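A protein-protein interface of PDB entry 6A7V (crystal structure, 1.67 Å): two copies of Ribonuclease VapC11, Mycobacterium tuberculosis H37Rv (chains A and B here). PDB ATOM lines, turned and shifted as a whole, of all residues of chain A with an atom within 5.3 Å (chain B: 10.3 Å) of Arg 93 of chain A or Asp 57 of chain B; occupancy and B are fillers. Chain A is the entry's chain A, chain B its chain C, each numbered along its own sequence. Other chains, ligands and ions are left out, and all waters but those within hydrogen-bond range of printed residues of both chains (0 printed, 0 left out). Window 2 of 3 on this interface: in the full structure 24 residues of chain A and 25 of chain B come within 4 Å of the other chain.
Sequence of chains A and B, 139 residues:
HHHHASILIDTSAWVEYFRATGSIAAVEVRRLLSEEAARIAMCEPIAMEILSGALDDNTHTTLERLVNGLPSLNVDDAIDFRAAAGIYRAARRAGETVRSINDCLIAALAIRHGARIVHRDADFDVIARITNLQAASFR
The backbone NH of Thr 59 of chain B lies within hydrogen-bond range of the side-chain carboxylate of Asp 56 of chain B (3.3 Å).
OD1 of Asp 56 of chain B sits at hydrogen-bond distance from N of Asn 58 of chain B (2.7 Å).
The backbone carbonyl oxygen (O) of Asp 57 of chain B lies within hydrogen-bond range of the side-chain hydroxyl (OG1) of Thr 61 of chain B, 2.9 Å away.
Of the printed residues of chain B, Arg 89 of chain A touches Leu 51, Ser 52, Ala 54, Leu 55, Asp 56, Asp 57 and His 60.
No residue of chain B comes within 4 Å of Ala 90 of chain A.
No residue of chain B comes within 4 Å of Ala 91 of chain A.
Of the printed residues of chain B, Arg 92 of chain A touches Ser 52 (2.8 Å), Ala 54 (3.6 Å) and Leu 55 (3.4 Å).
No residue of chain B comes within 4 Å of Ala 94 of chain A.
Printed residues of chain A within 4 Å of Ala 54 of chain B: Arg 89 and Arg 92.
Of chain A, only Arg 89 and Arg 93 come within 4 Å of Asp 57 of chain B.
Of the printed residues of chain A, His 60 of chain B touches Arg 89 (3.4 Å).
Arg 65 of chain B touches none of the printed residues of chain A.
No position is printed for both chains.
Of the 12 pairs that touch across the chains among the printed residues, none has its exchanged pair printed and touching as well.
Of the 8 printed residues of chain A, 4 touch a printed residue of chain B.
Printed residues of chain A that touch a printed residue of chain B: Tyr 88, Arg 89, Arg 92 and Arg 93.
Hydrophobic or aromatic side chains of chain A within 4 Å of the printed part of chain B: Tyr 88.
Among the printed residues, Asp or Glu carboxylates within 4 Å of a Lys or Arg side-chain nitrogen of the other chain: Arg 89 of chain A with Asp 57 of chain B (2.7 Å) and Arg 93 of chain A with Asp 57 of chain B (2.9 Å).
The backbone carbonyl oxygen (O) of Ala 54 of chain B lies within hydrogen-bond range of the guanidinium group (NE) of Arg 89 of chain A.
OD1 of Asp 57 of chain B is in salt-bridge range of NH2 of Arg 89 of chain A.
The guanidinium group (NH2) of Arg 89 of chain A is in hydrogen-bond range of the backbone carbonyl oxygen (O) of Leu 55 of chain B (3.3 Å).
NH1 of Arg 92 of chain A lies within hydrogen-bond range of O of Ser 52 of chain B (2.8 Å).
The guanidinium group (NH2) of Arg 93 of chain A lies within salt-bridge range of the side-chain carboxylate (OD2) of Asp 57 of chain B (2.9 Å).
Tyr 88 of chain A touches Ser 52 of chain B.
Arg 89 of chain A touches Leu 51 of chain B (CD to O, 3.3 Å).
O of Ser 52 of chain B touches CG of Arg 89 of chain A, 3.9 Å away.
NH2 of Arg 89 of chain A touches O of Asp 56 of chain B (3.99 Å).
His 60 of chain B touches Arg 89 of chain A.
Arg 92 of chain A touches Ala 54 of chain B (NH2 to O, 3.6 Å).
Arg 92 of chain A touches Leu 55 of chain B (CZ to CD1, 3.4 Å).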
ATOM      1  N   TYR A  88     -11.526 -17.054  32.188  1.00  0.00           N
ATOM      2  CA  TYR A  88     -12.283 -18.292  32.323  1.00  0.00           C
ATOM      3  C   TYR A  88     -11.797 -19.297  31.273  1.00  0.00           C
ATOM      4  O   TYR A  88     -11.551 -20.495  31.585  1.00  0.00           O
ATOM      5  CB  TYR A  88     -13.790 -18.039  32.183  1.00  0.00           C
ATOM      6  CG  TYR A  88     -14.654 -19.224  32.558  1.00  0.00           C
ATOM      7  CD1 TYR A  88     -15.082 -19.406  33.869  1.00  0.00           C
ATOM      8  CD2 TYR A  88     -15.043 -20.162  31.606  1.00  0.00           C
ATOM      9  CE1 TYR A  88     -15.871 -20.487  34.225  1.00  0.00           C
ATOM     10  CE2 TYR A  88     -15.832 -21.246  31.953  1.00  0.00           C
ATOM     11  CZ  TYR A  88     -16.246 -21.403  33.266  1.00  0.00           C
ATOM     12  OH  TYR A  88     -17.031 -22.472  33.627  1.00  0.00           O
ATOM     13  N   ARG A  89     -11.688 -18.789  30.042  1.00  0.00           N
ATOM     14  CA  ARG A  89     -11.302 -19.638  28.921  1.00  0.00           C
ATOM     15  C   ARG A  89      -9.909 -20.196  29.178  1.00  0.00           C
ATOM     16  O   ARG A  89      -9.653 -21.395  28.927  1.00  0.00           O
ATOM     17  CB  ARG A  89     -11.458 -18.927  27.576  1.00  0.00           C
ATOM     18  CG  ARG A  89     -12.928 -18.642  27.264  1.00  0.00           C
ATOM     19  CD  ARG A  89     -13.157 -18.143  25.849  1.00  0.00           C
ATOM     20  NE  ARG A  89     -13.058 -19.227  24.866  1.00  0.00           N
ATOM     21  CZ  ARG A  89     -12.102 -19.354  23.948  1.00  0.00           C
ATOM     22  NH1 ARG A  89     -11.123 -18.460  23.836  1.00  0.00           N
ATOM     23  NH2 ARG A  89     -12.131 -20.391  23.114  1.00  0.00           N
ATOM     24  N   ALA A  90      -9.020 -19.330  29.643  1.00  0.00           N
ATOM     25  CA  ALA A  90      -7.630 -19.737  29.902  1.00  0.00           C
ATOM     26  C   ALA A  90      -7.591 -20.806  30.964  1.00  0.00           C
ATOM     27  O   ALA A  90      -6.867 -21.781  30.840  1.00  0.00           O
ATOM     28  CB  ALA A  90      -6.777 -18.542  30.288  1.00  0.00           C
ATOM     29  N   ALA A  91      -8.407 -20.640  31.995  1.00  0.00           N
ATOM     30  CA  ALA A  91      -8.502 -21.609  33.092  1.00  0.00           C
ATOM     31  C   ALA A  91      -8.965 -22.978  32.554  1.00  0.00           C
ATOM     32  O   ALA A  91      -8.376 -24.005  32.893  1.00  0.00           O
ATOM     33  CB  ALA A  91      -9.439 -21.120  34.174  1.00  0.00           C
ATOM     34  N   ARG A  92      -9.997 -22.943  31.689  1.00  0.00           N
ATOM     35  CA  ARG A  92     -10.509 -24.170  31.166  1.00  0.00           C
ATOM     36  C   ARG A  92      -9.444 -24.854  30.302  1.00  0.00           C
ATOM     37  O   ARG A  92      -9.268 -26.103  30.394  1.00  0.00           O
ATOM     38  CB  ARG A  92     -11.830 -24.028  30.417  1.00  0.00           C
ATOM     39  CG  ARG A  92     -12.520 -25.384  30.255  1.00  0.00           C
ATOM     40  CD  ARG A  92     -13.710 -25.359  29.314  1.00  0.00           C
ATOM     41  NE  ARG A  92     -13.564 -24.322  28.298  1.00  0.00           N
ATOM     42  CZ  ARG A  92     -14.364 -23.266  28.156  1.00  0.00           C
ATOM     43  NH1 ARG A  92     -15.423 -23.092  28.942  1.00  0.00           N
ATOM     44  NH2 ARG A  92     -14.110 -22.383  27.196  1.00  0.00           N
ATOM     45  N   ARG A  93      -8.719 -24.079  29.509  1.00  0.00           N
ATOM     46  CA  ARG A  93      -7.695 -24.647  28.657  1.00  0.00           C
ATOM     47  C   ARG A  93      -6.557 -25.216  29.491  1.00  0.00           C
ATOM     48  O   ARG A  93      -5.932 -26.128  29.010  1.00  0.00           O
ATOM     49  CB  ARG A  93      -7.195 -23.560  27.700  1.00  0.00           C
ATOM     50  CG  ARG A  93      -6.195 -24.016  26.657  1.00  0.00           C
ATOM     51  CD  ARG A  93      -5.997 -22.962  25.577  1.00  0.00           C
ATOM     52  NE  ARG A  93      -6.662 -23.334  24.326  1.00  0.00           N
ATOM     53  CZ  ARG A  93      -7.849 -22.898  23.901  1.00  0.00           C
ATOM     54  NH1 ARG A  93      -8.577 -22.035  24.611  1.00  0.00           N
ATOM     55  NH2 ARG A  93      -8.312 -23.337  22.731  1.00  0.00           N
ATOM     56  N   ALA A  94      -6.223 -24.624  30.649  1.00  0.00           N
ATOM     57  CA  ALA A  94      -5.232 -25.160  31.509  1.00  0.00           C
ATOM     58  C   ALA A  94      -5.677 -26.437  32.205  1.00  0.00           C
ATOM     59  O   ALA A  94      -4.932 -26.890  33.000  1.00  0.00           O
ATOM     60  CB  ALA A  94      -4.796 -24.113  32.528  1.00  0.00           C
ATOM     61  N   GLY A  95      -6.892 -26.932  31.995  1.00  0.00           N
ATOM     62  CA  GLY A  95      -7.399 -28.057  32.779  1.00  0.00           C
ATOM     63  C   GLY A  95      -7.716 -27.703  34.227  1.00  0.00           C
ATOM     64  O   GLY A  95      -7.712 -28.573  35.098  1.00  0.00           O
ATOM     65  N   LEU B  51     -19.089 -16.041  25.483  1.00  0.00           N
ATOM     66  CA  LEU B  51     -17.698 -16.274  25.131  1.00  0.00           C
ATOM     67  C   LEU B  51     -17.126 -17.413  26.002  1.00  0.00           C
ATOM     68  O   LEU B  51     -16.412 -18.260  25.495  1.00  0.00           O
ATOM     69  CB  LEU B  51     -16.889 -14.981  25.216  1.00  0.00           C
ATOM     70  CG  LEU B  51     -17.328 -13.900  24.219  1.00  0.00           C
ATOM     71  CD1 LEU B  51     -16.433 -12.678  24.323  1.00  0.00           C
ATOM     72  CD2 LEU B  51     -17.366 -14.410  22.779  1.00  0.00           C
ATOM     73  N   SER B  52     -17.551 -17.443  27.251  1.00  0.00           N
ATOM     74  CA  SER B  52     -16.944 -18.356  28.215  1.00  0.00           C
ATOM     75  C   SER B  52     -17.160 -19.792  27.803  1.00  0.00           C
ATOM     76  O   SER B  52     -16.252 -20.598  27.942  1.00  0.00           O
ATOM     77  CB  SER B  52     -17.454 -18.093  29.628  1.00  0.00           C
ATOM     78  OG  SER B  52     -16.919 -16.866  30.111  1.00  0.00           O
ATOM     79  N   GLY B  53     -18.329 -20.087  27.239  1.00  0.00           N
ATOM     80  CA  GLY B  53     -18.680 -21.438  26.825  1.00  0.00           C
ATOM     81  C   GLY B  53     -18.301 -21.806  25.410  1.00  0.00           C
ATOM     82  O   GLY B  53     -18.644 -22.893  24.972  1.00  0.00           O
ATOM     83  N   ALA B  54     -17.619 -20.916  24.692  1.00  0.00           N
ATOM     84  CA  ALA B  54     -17.102 -21.236  23.363  1.00  0.00           C
ATOM     85  C   ALA B  54     -15.729 -21.902  23.499  1.00  0.00           C
ATOM     86  O   ALA B  54     -14.746 -21.235  23.812  1.00  0.00           O
ATOM     87  CB  ALA B  54     -16.997 -19.978  22.519  1.00  0.00           C
ATOM     88  N   LEU B  55     -15.676 -23.211  23.269  1.00  0.00           N
ATOM     89  CA  LEU B  55     -14.437 -23.978  23.443  1.00  0.00           C
ATOM     90  C   LEU B  55     -13.503 -23.838  22.242  1.00  0.00           C
ATOM     91  O   LEU B  55     -12.313 -23.598  22.407  1.00  0.00           O
ATOM     92  CB  LEU B  55     -14.744 -25.460  23.715  1.00  0.00           C
ATOM     93  CG  LEU B  55     -15.016 -25.840  25.176  1.00  0.00           C
ATOM     94  CD1 LEU B  55     -16.105 -24.979  25.802  1.00  0.00           C
ATOM     95  CD2 LEU B  55     -15.376 -27.317  25.279  1.00  0.00           C
ATOM     96  N   ASP B  56     -14.050 -23.994  21.039  1.00  0.00           N
ATOM     97  CA  ASP B  56     -13.300 -23.795  19.795  1.00  0.00           C
ATOM     98  C   ASP B  56     -12.959 -22.311  19.611  1.00  0.00           C
ATOM     99  O   ASP B  56     -13.849 -21.464  19.677  1.00  0.00           O
ATOM    100  CB  ASP B  56     -14.142 -24.310  18.618  1.00  0.00           C
ATOM    101  CG  ASP B  56     -13.399 -24.287  17.291  1.00  0.00           C
ATOM    102  OD1 ASP B  56     -12.743 -23.277  16.979  1.00  0.00           O
ATOM    103  OD2 ASP B  56     -13.500 -25.280  16.539  1.00  0.00           O
ATOM    104  N   ASP B  57     -11.681 -22.000  19.372  1.00  0.00           N
ATOM    105  CA  ASP B  57     -11.216 -20.618  19.255  1.00  0.00           C
ATOM    106  C   ASP B  57     -11.720 -19.938  17.984  1.00  0.00           C
ATOM    107  O   ASP B  57     -11.831 -18.683  17.938  1.00  0.00           O
ATOM    108  CB  ASP B  57      -9.680 -20.555  19.307  1.00  0.00           C
ATOM    109  CG  ASP B  57      -9.109 -20.896  20.688  1.00  0.00           C
ATOM    110  OD1 ASP B  57      -9.832 -20.789  21.705  1.00  0.00           O
ATOM    111  OD2 ASP B  57      -7.917 -21.268  20.762  1.00  0.00           O
ATOM    112  N   ASN B  58     -11.978 -20.724  16.949  1.00  0.00           N
ATOM    113  CA  ASN B  58     -12.571 -20.163  15.731  1.00  0.00           C
ATOM    114  C   ASN B  58     -14.021 -19.725  16.014  1.00  0.00           C
ATOM    115  O   ASN B  58     -14.437 -18.621  15.653  1.00  0.00           O
ATOM    116  CB  ASN B  58     -12.515 -21.187  14.594  1.00  0.00           C
ATOM    117  CG  ASN B  58     -11.097 -21.616  14.276  1.00  0.00           C
ATOM    118  OD1 ASN B  58     -10.235 -20.780  14.015  1.00  0.00           O
ATOM    119  ND2 ASN B  58     -10.845 -22.922  14.308  1.00  0.00           N
ATOM    120  N   THR B  59     -14.760 -20.629  16.649  1.00  0.00           N
ATOM    121  CA  THR B  59     -16.132 -20.332  17.044  1.00  0.00           C
ATOM    122  C   THR B  59     -16.163 -19.127  17.965  1.00  0.00           C
ATOM    123  O   THR B  59     -17.042 -18.280  17.834  1.00  0.00           O
ATOM    124  CB  THR B  59     -16.778 -21.547  17.733  1.00  0.00           C
ATOM    125  OG1 THR B  59     -16.772 -22.665  16.831  1.00  0.00           O
ATOM    126  CG2 THR B  59     -18.210 -21.246  18.155  1.00  0.00           C
ATOM    127  N   HIS B  60     -15.224 -19.092  18.918  1.00  0.00           N
ATOM    128  CA  HIS B  60     -15.119 -17.975  19.853  1.00  0.00           C
ATOM    129  C   HIS B  60     -14.937 -16.648  19.103  1.00  0.00           C
ATOM    130  O   HIS B  60     -15.584 -15.667  19.438  1.00  0.00           O
ATOM    131  CB  HIS B  60     -13.961 -18.196  20.837  1.00  0.00           C
ATOM    132  CG  HIS B  60     -13.722 -17.047  21.769  1.00  0.00           C
ATOM    133  ND1 HIS B  60     -12.812 -16.048  21.499  1.00  0.00           N
ATOM    134  CD2 HIS B  60     -14.274 -16.737  22.968  1.00  0.00           C
ATOM    135  CE1 HIS B  60     -12.812 -15.173  22.489  1.00  0.00           C
ATOM    136  NE2 HIS B  60     -13.691 -15.568  23.394  1.00  0.00           N
ATOM    137  N   THR B  61     -14.077 -16.638  18.097  1.00  0.00           N
ATOM    138  CA  THR B  61     -13.826 -15.503  17.273  1.00  0.00           C
ATOM    139  C   THR B  61     -15.129 -14.987  16.599  1.00  0.00           C
ATOM    140  O   THR B  61     -15.462 -13.796  16.620  1.00  0.00           O
ATOM    141  CB  THR B  61     -12.717 -15.781  16.233  1.00  0.00           C
ATOM    142  OG1 THR B  61     -11.477 -15.999  16.918  1.00  0.00           O
ATOM    143  CG2 THR B  61     -12.549 -14.601  15.272  1.00  0.00           C
ATOM    144  N   THR B  62     -15.852 -15.946  16.054  1.00  0.00           N
ATOM    145  CA  THR B  62     -17.125 -15.675  15.403  1.00  0.00           C
ATOM    146  C   THR B  62     -18.115 -15.030  16.388  1.00  0.00           C
ATOM    147  O   THR B  62     -18.796 -14.068  16.046  1.00  0.00           O
ATOM    148  CB  THR B  62     -17.705 -16.959  14.789  1.00  0.00           C
ATOM    149  OG1 THR B  62     -16.769 -17.476  13.837  1.00  0.00           O
ATOM    150  CG2 THR B  62     -19.017 -16.683  14.096  1.00  0.00           C
ATOM    151  N   LEU B  63     -18.174 -15.605  17.596  1.00  0.00           N
ATOM    152  CA  LEU B  63     -19.029 -15.118  18.636  1.00  0.00           C
ATOM    153  C   LEU B  63     -18.678 -13.696  19.066  1.00  0.00           C
ATOM    154  O   LEU B  63     -19.521 -12.896  19.388  1.00  0.00           O
ATOM    155  CB  LEU B  63     -19.221 -16.117  19.778  1.00  0.00           C
ATOM    156  CG  LEU B  63     -19.917 -17.415  19.320  1.00  0.00           C
ATOM    157  CD1 LEU B  63     -20.041 -18.373  20.497  1.00  0.00           C
ATOM    158  CD2 LEU B  63     -21.289 -17.185  18.700  1.00  0.00           C
ATOM    159  N   GLU B  64     -17.404 -13.426  19.090  1.00  0.00           N
ATOM    160  CA  GLU B  64     -16.873 -12.078  19.386  1.00  0.00           C
ATOM    161  C   GLU B  64     -17.408 -11.096  18.364  1.00  0.00           C
ATOM    162  O   GLU B  64     -17.786 -10.005  18.784  1.00  0.00           O
ATOM    163  CB  GLU B  64     -15.357 -12.046  19.373  1.00  0.00           C
ATOM    164  CG  GLU B  64     -14.735 -12.451  20.671  1.00  0.00           C
ATOM    165  CD  GLU B  64     -13.273 -12.082  20.736  1.00  0.00           C
ATOM    166  OE1 GLU B  64     -12.864 -11.438  21.728  1.00  0.00           O
ATOM    167  OE2 GLU B  64     -12.545 -12.414  19.793  1.00  0.00           O
ATOM    168  N   ARG B  65     -17.474 -11.436  17.100  1.00  0.00           N
ATOM    169  CA  ARG B  65     -18.045 -10.582  16.094  1.00  0.00           C
ATOM    170  C   ARG B  65     -19.496 -10.213  16.409  1.00  0.00           C
ATOM    171  O   ARG B  65     -19.897  -9.051  16.313  1.00  0.00           O
ATOM    172  CB  ARG B  65     -17.984 -11.215  14.695  1.00  0.00           C
ATOM    173  CG  ARG B  65     -16.599 -11.248  14.068  1.00  0.00           C
ATOM    174  CD  ARG B  65     -16.615 -11.987  12.733  1.00  0.00           C
ATOM    175  NE  ARG B  65     -17.496 -11.343  11.759  1.00  0.00           N
ATOM    176  CZ  ARG B  65     -17.930 -11.906  10.630  1.00  0.00           C
ATOM    177  NH1 ARG B  65     -17.585 -13.148  10.303  1.00  0.00           N
ATOM    178  NH2 ARG B  65     -18.729 -11.221   9.819  1.00  0.00           N
